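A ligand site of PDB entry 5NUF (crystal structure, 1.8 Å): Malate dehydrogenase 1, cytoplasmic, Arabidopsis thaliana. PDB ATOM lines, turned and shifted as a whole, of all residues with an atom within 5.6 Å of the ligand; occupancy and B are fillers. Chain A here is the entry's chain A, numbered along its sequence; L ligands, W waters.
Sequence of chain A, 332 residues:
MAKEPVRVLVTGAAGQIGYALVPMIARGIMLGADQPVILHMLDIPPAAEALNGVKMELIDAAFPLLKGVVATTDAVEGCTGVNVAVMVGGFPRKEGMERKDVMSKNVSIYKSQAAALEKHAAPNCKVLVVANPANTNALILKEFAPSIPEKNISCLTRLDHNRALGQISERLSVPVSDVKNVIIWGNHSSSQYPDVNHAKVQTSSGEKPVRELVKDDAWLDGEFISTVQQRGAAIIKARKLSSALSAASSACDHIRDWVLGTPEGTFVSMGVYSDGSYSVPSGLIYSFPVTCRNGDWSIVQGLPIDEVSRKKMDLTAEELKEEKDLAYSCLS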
ATOM      1  N   THR A  11      35.359 -29.789   5.267  1.00  0.00           N
ATOM      2  CA  THR A  11      35.591 -29.861   6.704  1.00  0.00           C
ATOM      3  C   THR A  11      34.305 -30.222   7.392  1.00  0.00           C
ATOM      4  O   THR A  11      33.231 -30.057   6.803  1.00  0.00           O
ATOM      5  CB  THR A  11      36.182 -28.563   7.287  1.00  0.00           C
ATOM      6  OG1 THR A  11      35.183 -27.554   7.391  1.00  0.00           O
ATOM      7  CG2 THR A  11      37.377 -28.102   6.463  1.00  0.00           C
ATOM      8  N   GLY A  12      34.352 -30.695   8.624  1.00  0.00           N
ATOM      9  CA  GLY A  12      33.163 -31.281   9.286  1.00  0.00           C
ATOM     10  C   GLY A  12      32.662 -32.540   8.616  1.00  0.00           C
ATOM     11  O   GLY A  12      31.468 -32.891   8.725  1.00  0.00           O
ATOM     12  N   ALA A  13      33.575 -33.260   7.909  1.00  0.00           N
ATOM     13  CA  ALA A  13      33.187 -34.339   7.035  1.00  0.00           C
ATOM     14  C   ALA A  13      32.543 -35.541   7.714  1.00  0.00           C
ATOM     15  O   ALA A  13      31.828 -36.274   7.076  1.00  0.00           O
ATOM     16  CB  ALA A  13      34.345 -34.804   6.170  1.00  0.00           C
ATOM     17  N   ALA A  14      32.798 -35.767   8.975  1.00  0.00           N
ATOM     18  CA  ALA A  14      32.167 -36.884   9.689  1.00  0.00           C
ATOM     19  C   ALA A  14      30.814 -36.541  10.260  1.00  0.00           C
ATOM     20  O   ALA A  14      30.208 -37.369  10.942  1.00  0.00           O
ATOM     21  CB  ALA A  14      33.097 -37.429  10.783  1.00  0.00           C
ATOM     22  N   GLY A  15      30.324 -35.331  10.009  1.00  0.00           N
ATOM     23  CA  GLY A  15      29.010 -34.968  10.507  1.00  0.00           C
ATOM     24  C   GLY A  15      27.880 -35.201   9.522  1.00  0.00           C
ATOM     25  O   GLY A  15      28.044 -35.811   8.494  1.00  0.00           O
ATOM     26  N   GLN A  16      26.720 -34.682   9.887  1.00  0.00           N
ATOM     27  CA  GLN A  16      25.486 -34.941   9.152  1.00  0.00           C
ATOM     28  C   GLN A  16      25.542 -34.363   7.744  1.00  0.00           C
ATOM     29  O   GLN A  16      25.265 -35.072   6.737  1.00  0.00           O
ATOM     30  CB  GLN A  16      24.338 -34.302   9.945  1.00  0.00           C
ATOM     31  CG  GLN A  16      23.017 -34.829   9.514  1.00  0.00           C
ATOM     32  CD  GLN A  16      21.751 -34.004   9.968  1.00  0.00           C
ATOM     33  OE1 GLN A  16      20.671 -34.535   9.775  1.00  0.00           O
ATOM     34  NE2 GLN A  16      21.896 -32.749  10.552  1.00  0.00           N
ATOM     35  N   ILE A  17      25.921 -33.098   7.630  1.00  0.00           N
ATOM     36  CA  ILE A  17      26.005 -32.473   6.293  1.00  0.00           C
ATOM     37  C   ILE A  17      27.136 -33.079   5.494  1.00  0.00           C
ATOM     38  O   ILE A  17      26.987 -33.359   4.305  1.00  0.00           O
ATOM     39  CB  ILE A  17      26.143 -30.962   6.378  1.00  0.00           C
ATOM     40  CG1 ILE A  17      24.857 -30.357   6.876  1.00  0.00           C
ATOM     41  CG2 ILE A  17      26.498 -30.361   5.024  1.00  0.00           C
ATOM     42  CD1 ILE A  17      24.940 -28.892   7.202  1.00  0.00           C
ATOM     43  N   GLY A  18      28.246 -33.357   6.140  1.00  0.00           N
ATOM     44  CA  GLY A  18      29.342 -33.969   5.510  1.00  0.00           C
ATOM     45  C   GLY A  18      29.017 -35.309   4.834  1.00  0.00           C
ATOM     46  O   GLY A  18      29.401 -35.565   3.671  1.00  0.00           O
ATOM     47  N   LEU A  42      38.149 -33.396   6.369  1.00  0.00           N
ATOM     48  CA  LEU A  42      38.732 -33.014   7.639  1.00  0.00           C
ATOM     49  C   LEU A  42      37.687 -33.016   8.766  1.00  0.00           C
ATOM     50  O   LEU A  42      36.583 -32.459   8.633  1.00  0.00           O
ATOM     51  CB  LEU A  42      39.305 -31.594   7.497  1.00  0.00           C
ATOM     52  CG  LEU A  42      39.940 -31.017   8.794  1.00  0.00           C
ATOM     53  CD1 LEU A  42      41.251 -31.740   9.174  1.00  0.00           C
ATOM     54  CD2 LEU A  42      40.251 -29.550   8.593  1.00  0.00           C
ATOM     55  N   ASP A  43      38.024 -33.650   9.878  1.00  0.00           N
ATOM     56  CA  ASP A  43      37.210 -33.577  11.081  1.00  0.00           C
ATOM     57  C   ASP A  43      38.155 -33.532  12.281  1.00  0.00           C
ATOM     58  O   ASP A  43      39.333 -33.199  12.107  1.00  0.00           O
ATOM     59  CB  ASP A  43      36.173 -34.701  11.132  1.00  0.00           C
ATOM     60  CG  ASP A  43      34.903 -34.296  11.854  1.00  0.00           C
ATOM     61  OD1 ASP A  43      34.982 -34.081  13.088  1.00  0.00           O
ATOM     62  OD2 ASP A  43      33.831 -34.067  11.184  1.00  0.00           O
ATOM     63  N   ILE A  44      37.667 -33.830  13.457  1.00  0.00           N
ATOM     64  CA  ILE A  44      38.479 -33.685  14.660  1.00  0.00           C
ATOM     65  C   ILE A  44      38.742 -35.056  15.290  1.00  0.00           C
ATOM     66  O   ILE A  44      38.039 -36.022  15.004  1.00  0.00           O
ATOM     67  CB  ILE A  44      37.917 -32.631  15.670  1.00  0.00           C
ATOM     68  CG1 ILE A  44      36.428 -32.874  15.910  1.00  0.00           C
ATOM     69  CG2 ILE A  44      38.265 -31.218  15.230  1.00  0.00           C
ATOM     70  CD1 ILE A  44      35.835 -32.224  17.156  1.00  0.00           C
ATOM     71  N   ALA A  47      36.234 -37.867  16.195  1.00  0.00           N
ATOM     72  CA  ALA A  47      35.500 -38.478  15.077  1.00  0.00           C
ATOM     73  C   ALA A  47      36.423 -39.255  14.098  1.00  0.00           C
ATOM     74  O   ALA A  47      36.011 -39.592  12.984  1.00  0.00           O
ATOM     75  CB  ALA A  47      34.745 -37.343  14.340  1.00  0.00           C
ATOM     76  N   VAL A  88      32.265 -27.023   6.687  1.00  0.00           N
ATOM     77  CA  VAL A  88      31.112 -27.448   7.409  1.00  0.00           C
ATOM     78  C   VAL A  88      31.442 -27.757   8.888  1.00  0.00           C
ATOM     79  O   VAL A  88      30.560 -27.970   9.702  1.00  0.00           O
ATOM     80  CB  VAL A  88      30.427 -28.650   6.709  1.00  0.00           C
ATOM     81  CG1 VAL A  88      29.001 -28.776   7.137  1.00  0.00           C
ATOM     82  CG2 VAL A  88      30.441 -28.490   5.200  1.00  0.00           C
ATOM     83  N   GLY A  89      32.714 -27.710   9.236  1.00  0.00           N
ATOM     84  CA  GLY A  89      33.158 -27.994  10.589  1.00  0.00           C
ATOM     85  C   GLY A  89      32.614 -26.981  11.593  1.00  0.00           C
ATOM     86  O   GLY A  89      32.638 -25.736  11.369  1.00  0.00           O
ATOM     87  N   GLY A  90      31.978 -27.504  12.647  1.00  0.00           N
ATOM     88  CA  GLY A  90      31.410 -26.672  13.650  1.00  0.00           C
ATOM     89  C   GLY A  90      30.594 -27.415  14.630  1.00  0.00           C
ATOM     90  O   GLY A  90      30.587 -28.686  14.638  1.00  0.00           O
ATOM     91  N   PHE A  91      29.830 -26.644  15.400  1.00  0.00           N
ATOM     92  CA  PHE A  91      28.964 -27.171  16.440  1.00  0.00           C
ATOM     93  C   PHE A  91      27.617 -26.489  16.324  1.00  0.00           C
ATOM     94  O   PHE A  91      27.496 -25.265  16.580  1.00  0.00           O
ATOM     95  CB  PHE A  91      29.556 -26.904  17.845  1.00  0.00           C
ATOM     96  CG  PHE A  91      30.887 -27.568  18.044  1.00  0.00           C
ATOM     97  CD1 PHE A  91      30.965 -28.886  18.430  1.00  0.00           C
ATOM     98  CD2 PHE A  91      32.067 -26.863  17.827  1.00  0.00           C
ATOM     99  CE1 PHE A  91      32.211 -29.535  18.571  1.00  0.00           C
ATOM    100  CE2 PHE A  91      33.315 -27.492  17.973  1.00  0.00           C
ATOM    101  CZ  PHE A  91      33.393 -28.810  18.358  1.00  0.00           C
ATOM    102  N   PRO A  92      26.578 -27.241  15.916  1.00  0.00           N
ATOM    103  CA  PRO A  92      25.232 -26.682  15.801  1.00  0.00           C
ATOM    104  C   PRO A  92      24.683 -26.343  17.195  1.00  0.00           C
ATOM    105  O   PRO A  92      25.061 -27.006  18.164  1.00  0.00           O
ATOM    106  CB  PRO A  92      24.417 -27.795  15.164  1.00  0.00           C
ATOM    107  CG  PRO A  92      25.171 -29.049  15.464  1.00  0.00           C
ATOM    108  CD  PRO A  92      26.624 -28.654  15.540  1.00  0.00           C
ATOM    109  N   ARG A  93      23.849 -25.308  17.268  1.00  0.00           N
ATOM    110  CA  ARG A  93      23.267 -24.868  18.553  1.00  0.00           C
ATOM    111  C   ARG A  93      22.398 -25.984  19.111  1.00  0.00           C
ATOM    112  O   ARG A  93      21.624 -26.573  18.359  1.00  0.00           O
ATOM    113  CB  ARG A  93      22.446 -23.575  18.354  1.00  0.00           C
ATOM    114  CG  ARG A  93      21.792 -23.037  19.627  1.00  0.00           C
ATOM    115  CD  ARG A  93      21.177 -21.669  19.450  1.00  0.00           C
ATOM    116  NE  ARG A  93      21.086 -20.976  20.744  1.00  0.00           N
ATOM    117  CZ  ARG A  93      20.848 -19.670  20.920  1.00  0.00           C
ATOM    118  NH1 ARG A  93      20.618 -18.836  19.902  1.00  0.00           N
ATOM    119  NH2 ARG A  93      20.816 -19.186  22.166  1.00  0.00           N
ATOM    120  N   ASN A 106      32.349 -21.871  17.459  1.00  0.00           N
ATOM    121  CA  ASN A 106      32.466 -21.887  15.992  1.00  0.00           C
ATOM    122  C   ASN A 106      33.456 -20.909  15.424  1.00  0.00           C
ATOM    123  O   ASN A 106      34.265 -21.288  14.599  1.00  0.00           O
ATOM    124  CB  ASN A 106      31.053 -21.700  15.393  1.00  0.00           C
ATOM    125  CG  ASN A 106      30.204 -22.900  15.654  1.00  0.00           C
ATOM    126  OD1 ASN A 106      30.459 -23.899  15.091  1.00  0.00           O
ATOM    127  ND2 ASN A 106      29.252 -22.834  16.577  1.00  0.00           N
ATOM    128  N   ILE A 109      37.168 -21.897  15.289  1.00  0.00           N
ATOM    129  CA  ILE A 109      37.539 -22.842  14.247  1.00  0.00           C
ATOM    130  C   ILE A 109      38.067 -22.072  13.030  1.00  0.00           C
ATOM    131  O   ILE A 109      39.057 -22.458  12.425  1.00  0.00           O
ATOM    132  CB  ILE A 109      36.332 -23.731  13.811  1.00  0.00           C
ATOM    133  CG1 ILE A 109      35.866 -24.547  14.976  1.00  0.00           C
ATOM    134  CG2 ILE A 109      36.691 -24.620  12.614  1.00  0.00           C
ATOM    135  CD1 ILE A 109      34.558 -25.270  14.679  1.00  0.00           C
ATOM    136  N   GLN A 113      41.649 -22.289  11.246  1.00  0.00           N
ATOM    137  CA  GLN A 113      41.746 -22.849   9.882  1.00  0.00           C
ATOM    138  C   GLN A 113      42.028 -21.878   8.774  1.00  0.00           C
ATOM    139  O   GLN A 113      42.462 -22.286   7.714  1.00  0.00           O
ATOM    140  CB  GLN A 113      40.531 -23.706   9.562  1.00  0.00           C
ATOM    141  CG  GLN A 113      40.429 -24.910  10.488  1.00  0.00           C
ATOM    142  CD  GLN A 113      39.151 -25.749  10.205  1.00  0.00           C
ATOM    143  OE1 GLN A 113      38.263 -25.343   9.438  1.00  0.00           O
ATOM    144  NE2 GLN A 113      39.047 -26.890  10.865  1.00  0.00           N
ATOM    145  N   VAL A 129      31.760 -21.250   3.210  1.00  0.00           N
ATOM    146  CA  VAL A 129      31.478 -21.515   4.595  1.00  0.00           C
ATOM    147  C   VAL A 129      30.027 -21.835   4.795  1.00  0.00           C
ATOM    148  O   VAL A 129      29.136 -21.023   4.522  1.00  0.00           O
ATOM    149  CB  VAL A 129      31.921 -20.353   5.498  1.00  0.00           C
ATOM    150  CG1 VAL A 129      31.616 -20.682   6.972  1.00  0.00           C
ATOM    151  CG2 VAL A 129      33.424 -20.084   5.345  1.00  0.00           C
ATOM    152  N   VAL A 130      29.759 -23.052   5.305  1.00  0.00           N
ATOM    153  CA  VAL A 130      28.400 -23.531   5.571  1.00  0.00           C
ATOM    154  C   VAL A 130      28.125 -23.448   7.063  1.00  0.00           C
ATOM    155  O   VAL A 130      27.041 -23.073   7.464  1.00  0.00           O
ATOM    156  CB  VAL A 130      28.263 -24.982   5.069  1.00  0.00           C
ATOM    157  CG1 VAL A 130      26.921 -25.607   5.476  1.00  0.00           C
ATOM    158  CG2 VAL A 130      28.545 -25.096   3.583  1.00  0.00           C
ATOM    159  N   ALA A 131      29.102 -23.800   7.898  1.00  0.00           N
ATOM    160  CA  ALA A 131      28.907 -23.812   9.312  1.00  0.00           C
ATOM    161  C   ALA A 131      28.362 -22.539   9.859  1.00  0.00           C
ATOM    162  O   ALA A 131      28.801 -21.472   9.454  1.00  0.00           O
ATOM    163  CB  ALA A 131      30.202 -24.198  10.050  1.00  0.00           C
ATOM    164  N   ASN A 132      27.470 -22.662  10.860  1.00  0.00           N
ATOM    165  CA  ASN A 132      26.817 -21.466  11.425  1.00  0.00           C
ATOM    166  C   ASN A 132      27.625 -20.898  12.585  1.00  0.00           C
ATOM    167  O   ASN A 132      28.343 -21.647  13.278  1.00  0.00           O
ATOM    168  CB  ASN A 132      25.369 -21.762  11.844  1.00  0.00           C
ATOM    169  CG  ASN A 132      24.423 -21.808  10.643  1.00  0.00           C
ATOM    170  OD1 ASN A 132      24.666 -21.060   9.668  1.00  0.00           O
ATOM    171  ND2 ASN A 132      23.427 -22.687  10.677  1.00  0.00           N
ATOM    172  N   ALA A 134      26.990 -18.627   9.508  1.00  0.00           N
ATOM    173  CA  ALA A 134      27.732 -18.760   8.268  1.00  0.00           C
ATOM    174  C   ALA A 134      28.461 -17.485   7.844  1.00  0.00           C
ATOM    175  O   ALA A 134      29.653 -17.526   7.529  1.00  0.00           O
ATOM    176  CB  ALA A 134      26.826 -19.259   7.151  1.00  0.00           C
ATOM    177  N   LEU A 156      27.144 -19.672   2.699  1.00  0.00           N
ATOM    178  CA  LEU A 156      25.951 -20.299   2.092  1.00  0.00           C
ATOM    179  C   LEU A 156      24.676 -19.632   2.520  1.00  0.00           C
ATOM    180  O   LEU A 156      24.209 -19.815   3.665  1.00  0.00           O
ATOM    181  CB  LEU A 156      25.857 -21.784   2.444  1.00  0.00           C
ATOM    182  CG  LEU A 156      24.826 -22.589   1.682  1.00  0.00           C
ATOM    183  CD1 LEU A 156      25.345 -22.802   0.274  1.00  0.00           C
ATOM    184  CD2 LEU A 156      24.588 -23.884   2.345  1.00  0.00           C
ATOM    185  N   LEU A 159      20.771 -22.228   0.470  1.00  0.00           N
ATOM    186  CA  LEU A 159      19.647 -22.986   1.040  1.00  0.00           C
ATOM    187  C   LEU A 159      18.473 -22.077   1.324  1.00  0.00           C
ATOM    188  O   LEU A 159      17.315 -22.424   1.030  1.00  0.00           O
ATOM    189  CB  LEU A 159      20.043 -23.783   2.264  1.00  0.00           C
ATOM    190  CG  LEU A 159      18.914 -24.537   2.997  1.00  0.00           C
ATOM    191  CD1 LEU A 159      18.210 -25.520   2.025  1.00  0.00           C
ATOM    192  CD2 LEU A 159      19.459 -25.314   4.158  1.00  0.00           C
ATOM    193  N   ASP A 160      18.726 -20.905   1.874  1.00  0.00           N
ATOM    194  CA  ASP A 160      17.642 -19.889   2.031  1.00  0.00           C
ATOM    195  C   ASP A 160      16.978 -19.582   0.681  1.00  0.00           C
ATOM    196  O   ASP A 160      15.724 -19.490   0.591  1.00  0.00           O
ATOM    197  CB  ASP A 160      18.205 -18.569   2.616  1.00  0.00           C
ATOM    198  CG  ASP A 160      18.874 -18.771   3.881  1.00  0.00           C
ATOM    199  OD1 ASP A 160      18.223 -19.303   4.871  1.00  0.00           O
ATOM    200  OD2 ASP A 160      20.043 -18.417   3.943  1.00  0.00           O
ATOM    201  N   ARG A 163      14.967 -22.491  -0.497  1.00  0.00           N
ATOM    202  CA  ARG A 163      13.781 -22.567   0.329  1.00  0.00           C
ATOM    203  C   ARG A 163      12.720 -21.623  -0.184  1.00  0.00           C
ATOM    204  O   ARG A 163      11.527 -21.964  -0.195  1.00  0.00           O
ATOM    205  CB  ARG A 163      14.090 -22.252   1.795  1.00  0.00           C
ATOM    206  CG  ARG A 163      14.628 -23.438   2.553  1.00  0.00           C
ATOM    207  CD  ARG A 163      15.328 -22.971   3.818  1.00  0.00           C
ATOM    208  NE  ARG A 163      15.766 -24.088   4.628  1.00  0.00           N
ATOM    209  CZ  ARG A 163      16.556 -23.973   5.713  1.00  0.00           C
ATOM    210  NH1 ARG A 163      17.055 -22.806   6.083  1.00  0.00           N
ATOM    211  NH2 ARG A 163      16.948 -25.045   6.393  1.00  0.00           N
ATOM    212  N   HIS A 188      22.469 -15.186   6.873  1.00  0.00           N
ATOM    213  CA  HIS A 188      21.837 -16.485   6.978  1.00  0.00           C
ATOM    214  C   HIS A 188      21.241 -16.614   8.394  1.00  0.00           C
ATOM    215  O   HIS A 188      21.900 -17.196   9.322  1.00  0.00           O
ATOM    216  CB  HIS A 188      22.823 -17.625   6.689  1.00  0.00           C
ATOM    217  CG  HIS A 188      22.192 -18.993   6.843  1.00  0.00           C
ATOM    218  ND1 HIS A 188      21.215 -19.451   5.990  1.00  0.00           N
ATOM    219  CD2 HIS A 188      22.409 -19.982   7.754  1.00  0.00           C
ATOM    220  CE1 HIS A 188      20.827 -20.642   6.391  1.00  0.00           C
ATOM    221  NE2 HIS A 188      21.522 -20.987   7.473  1.00  0.00           N
ATOM    222  N   SER A 242      19.001 -30.406  12.544  1.00  0.00           N
ATOM    223  CA  SER A 242      18.981 -29.356  11.499  1.00  0.00           C
ATOM    224  C   SER A 242      19.197 -29.980  10.108  1.00  0.00           C
ATOM    225  O   SER A 242      19.480 -31.164   9.976  1.00  0.00           O
ATOM    226  CB  SER A 242      19.967 -28.210  11.813  1.00  0.00           C
ATOM    227  OG  SER A 242      21.132 -28.723  12.325  1.00  0.00           O
ATOM    228  N   SER A 243      19.006 -29.166   9.080  1.00  0.00           N
ATOM    229  CA  SER A 243      18.971 -29.624   7.700  1.00  0.00           C
ATOM    230  C   SER A 243      20.305 -30.192   7.263  1.00  0.00           C
ATOM    231  O   SER A 243      21.354 -29.766   7.731  1.00  0.00           O
ATOM    232  CB  SER A 243      18.629 -28.425   6.790  1.00  0.00           C
ATOM    233  OG  SER A 243      19.635 -27.440   6.846  1.00  0.00           O
ATOM    234  N   ALA A 244      20.272 -31.135   6.355  1.00  0.00           N
ATOM    235  CA  ALA A 244      21.513 -31.755   5.900  1.00  0.00           C
ATOM    236  C   ALA A 244      21.432 -32.107   4.451  1.00  0.00           C
ATOM    237  O   ALA A 244      22.253 -31.646   3.640  1.00  0.00           O
ATOM    238  CB  ALA A 244      21.938 -32.937   6.800  1.00  0.00           C
ATOM    239  N   ALA A 247      20.937 -28.760   2.783  1.00  0.00           N
ATOM    240  CA  ALA A 247      22.143 -27.947   2.943  1.00  0.00           C
ATOM    241  C   ALA A 247      23.273 -28.441   2.019  1.00  0.00           C
ATOM    242  O   ALA A 247      23.891 -27.645   1.283  1.00  0.00           O
ATOM    243  CB  ALA A 247      22.588 -27.954   4.401  1.00  0.00           C
HETATM  244  P1  LIG L   1      27.332 -32.070  12.872  1.00  0.00           P
HETATM  245  O1  LIG L   1      26.676 -33.362  12.456  1.00  0.00           O
HETATM  246  O2  LIG L   1      27.661 -31.810  14.291  1.00  0.00           O
HETATM  247  O3  LIG L   1      28.687 -31.919  12.014  1.00  0.00           O
HETATM  248  C1  LIG L   1      29.723 -30.979  12.269  1.00  0.00           C
HETATM  249  C2  LIG L   1      31.066 -31.713  12.274  1.00  0.00           C
HETATM  250  O4  LIG L   1      32.050 -30.660  12.420  1.00  0.00           O
HETATM  251  C3  LIG L   1      31.269 -32.760  13.419  1.00  0.00           C
HETATM  252  O5  LIG L   1      31.650 -34.081  12.857  1.00  0.00           O
HETATM  253  C4  LIG L   1      32.415 -32.139  14.203  1.00  0.00           C
HETATM  254  O6  LIG L   1      33.190 -33.197  14.781  1.00  0.00           O
HETATM  255  C5  LIG L   1      33.089 -31.279  13.126  1.00  0.00           C
HETATM  256  N1  LIG L   1      34.024 -30.305  13.641  1.00  0.00           N
HETATM  257  C6  LIG L   1      33.988 -29.679  14.827  1.00  0.00           C
HETATM  258  N2  LIG L   1      35.102 -28.898  14.973  1.00  0.00           N
HETATM  259  C7  LIG L   1      35.851 -29.071  13.849  1.00  0.00           C
HETATM  260  C8  LIG L   1      37.121 -28.603  13.318  1.00  0.00           C
HETATM  261  N3  LIG L   1      37.878 -27.773  14.026  1.00  0.00           N
HETATM  262  N4  LIG L   1      37.551 -28.976  12.110  1.00  0.00           N
HETATM  263  C9  LIG L   1      36.792 -29.846  11.396  1.00  0.00           C
HETATM  264  N5  LIG L   1      35.618 -30.390  11.802  1.00  0.00           N
HETATM  265  C10 LIG L   1      35.121 -30.009  12.984  1.00  0.00           C
HETATM  266  O7  LIG L   1      26.523 -30.780  12.318  1.00  0.00           O
HETATM  267  P2  LIG L   1      25.791 -30.695  10.864  1.00  0.00           P
HETATM  268  O8  LIG L   1      24.341 -30.977  11.081  1.00  0.00           O
HETATM  269  O9  LIG L   1      26.586 -31.310   9.755  1.00  0.00           O
HETATM  270  O10 LIG L   1      25.826 -29.105  10.696  1.00  0.00           O
HETATM  271  C11 LIG L   1      27.107 -28.546  10.466  1.00  0.00           C
HETATM  272  C12 LIG L   1      27.100 -27.034  10.475  1.00  0.00           C
HETATM  273  O11 LIG L   1      26.346 -26.456   9.363  1.00  0.00           O
HETATM  274  C13 LIG L   1      26.492 -26.434  11.732  1.00  0.00           C
HETATM  275  O12 LIG L   1      27.260 -25.243  12.164  1.00  0.00           O
HETATM  276  C14 LIG L   1      25.131 -26.035  11.304  1.00  0.00           C
HETATM  277  O13 LIG L   1      24.476 -25.114  12.110  1.00  0.00           O
HETATM  278  C15 LIG L   1      25.394 -25.503   9.910  1.00  0.00           C
HETATM  279  N6  LIG L   1      24.307 -25.408   8.952  1.00  0.00           N
HETATM  280  C16 LIG L   1      24.300 -24.424   8.051  1.00  0.00           C
HETATM  281  C17 LIG L   1      23.336 -24.350   7.051  1.00  0.00           C
HETATM  282  C18 LIG L   1      23.405 -23.255   6.064  1.00  0.00           C
HETATM  283  O14 LIG L   1      24.402 -22.410   5.994  1.00  0.00           O
HETATM  284  N7  LIG L   1      22.483 -23.134   5.197  1.00  0.00           N
HETATM  285  C19 LIG L   1      22.326 -25.323   7.048  1.00  0.00           C
HETATM  286  C20 LIG L   1      22.366 -26.303   8.034  1.00  0.00           C
HETATM  287  C21 LIG L   1      23.350 -26.336   8.961  1.00  0.00           C
HETATM  288  O   HOH W   1      21.811 -21.342   3.170  1.00  0.00           O
HETATM  289  O   HOH W   2      26.067 -32.277  16.336  1.00  0.00           O
HETATM  290  O   HOH W   3      29.563 -30.957  15.961  1.00  0.00           O
HETATM  291  O   HOH W   4      41.001 -27.805  12.704  1.00  0.00           O
HETATM  292  O   HOH W   5      23.113 -31.709  13.660  1.00  0.00           O
HETATM  293  O   HOH W   6      26.927 -35.683  13.787  1.00  0.00           O
HETATM  294  O   HOH W   7      36.649 -27.773  16.906  1.00  0.00           O
HETATM  295  O   HOH W   8      32.772 -33.923  17.208  1.00  0.00           O
HETATM  296  O   HOH W   9      22.540 -29.214  10.188  1.00  0.00           O
HETATM  297  O   HOH W  10      26.684 -23.781  14.499  1.00  0.00           O
HETATM  298  O   HOH W  11      28.717 -32.169   8.699  1.00  0.00           O
HETATM  299  O   HOH W  12      30.710 -36.085  14.374  1.00  0.00           O
HETATM  300  O   HOH W  13      22.196 -26.234  13.148  1.00  0.00           O
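The side-chain carboxylate (OD1) of Asp 43 lies within hydrogen-bond range of an oxygen (O6) of the ligand (2.6 Å). The side-chain amide nitrogen of Gln 113 lies within hydrogen-bond range of a nitrogen (N4) of the ligand, at 2.9 Å. An oxygen (O9) of the ligand sits at hydrogen-bond distance from the backbone NH (N) of Ile 17 (2.9 Å). N of Gln 16 sits at hydrogen-bond distance from O1 of the ligand, at 2.9 Å. An oxygen (O8) of the ligand sits at hydrogen-bond distance from the side-chain amide nitrogen (NE2) of Gln 16, at 3.1 Å. O12 of the ligand lies within hydrogen-bond range of N of Asn 132, at 2.9 Å. The side-chain amide nitrogen of Asn 132 sits at hydrogen-bond distance from an oxygen (O13) of the ligand (3.0 Å). An oxygen (O4) of the ligand is in hydrogen-bond range of the backbone NH (N) of Gly 90, 3.2 Å away. NE2 of His 188 lies close to N7 of the ligand (3.3 Å). The backbone NH (N) of Gly 15 sits at hydrogen-bond distance from an oxygen (O5) of the ligand. The backbone NH (N) of Gly 12 sits at hydrogen-bond distance from a nitrogen (N5) of the ligand (3.4 Å).
The backbone NH (N) of Ala 14 lies within hydrogen-bond range of the side-chain carboxylate (OD2) of Asp 43 (3.0 Å). The side-chain amide nitrogen (NE2) of Gln 16 is in hydrogen-bond range of the backbone carbonyl oxygen (O) of Ser 242, at 2.9 Å. ND1 of His 188 is in hydrogen-bond range of OD2 of Asp 160 (2.6 Å). N of Gly 89 sits at hydrogen-bond distance from OG1 of Thr 11 (3.1 Å). The backbone carbonyl oxygen (O) of Val 129 is in hydrogen-bond range of the backbone NH (N) of Leu 156, 3.0 Å away. The side-chain hydroxyl (OG1) of Thr 11 is in hydrogen-bond range of the backbone NH (N) of Val 88 (3.0 Å). The backbone NH (N) of Phe 91 sits at hydrogen-bond distance from the side-chain amide oxygen (OD1) of Asn 106 (2.8 Å). O of Leu 42 is in hydrogen-bond range of N of Ala 13, at 3.2 Å.
An oxygen (O14) of the ligand sits close to the backbone carbonyl oxygen (O) of Val 130 (3.1 Å). O14 of the ligand lies close to O of Leu 156 (3.5 Å). Merely in contact with the ligand: Ala 14, Leu 42, Ile 44, Val 88, Gly 89, Phe 91, Pro 92, Ile 109, Ala 131, Leu 159, Ser 243 and Ala 247. Within 4 Å of the ligand: Gly 12, Ala 14, Gly 15, Gln 16, Ile 17, Leu 42, Asp 43, Ile 44, Val 88, Gly 89, Gly 90, Phe 91, Pro 92, Ile 109, Gln 113, Val 130, Ala 131, Asn 132, Leu 156, Leu 159, His 188, Ser 243 and Ala 247.
Water W3 lies within hydrogen-bond range of O2 of the ligand and O of Gly 90. Water W9 lies within hydrogen-bond range of the side-chain hydroxyl (OG) of Ser 242, an oxygen (O8) of the ligand and the backbone carbonyl oxygen (O) of Ser 243. Water W13 lies within hydrogen-bond range of an oxygen (O13) of the ligand (2.7 Å) and the side-chain hydroxyl (OG) of Ser 242 (2.8 Å). Water W10 lies within hydrogen-bond range of O of Phe 91 (2.7 Å), O12 of the ligand (2.8 Å), O of Asn 132 (3.0 Å) and ND2 of Asn 106 (3.4 Å). Water W5 lies within hydrogen-bond range of an oxygen (O8) of the ligand (2.9 Å) and the side-chain amide nitrogen of Gln 16 (3.5 Å). Water W4 lies within hydrogen-bond range of the side-chain amide nitrogen of Gln 113 (2.8 Å) and a nitrogen (N3) of the ligand (3.4 Å).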
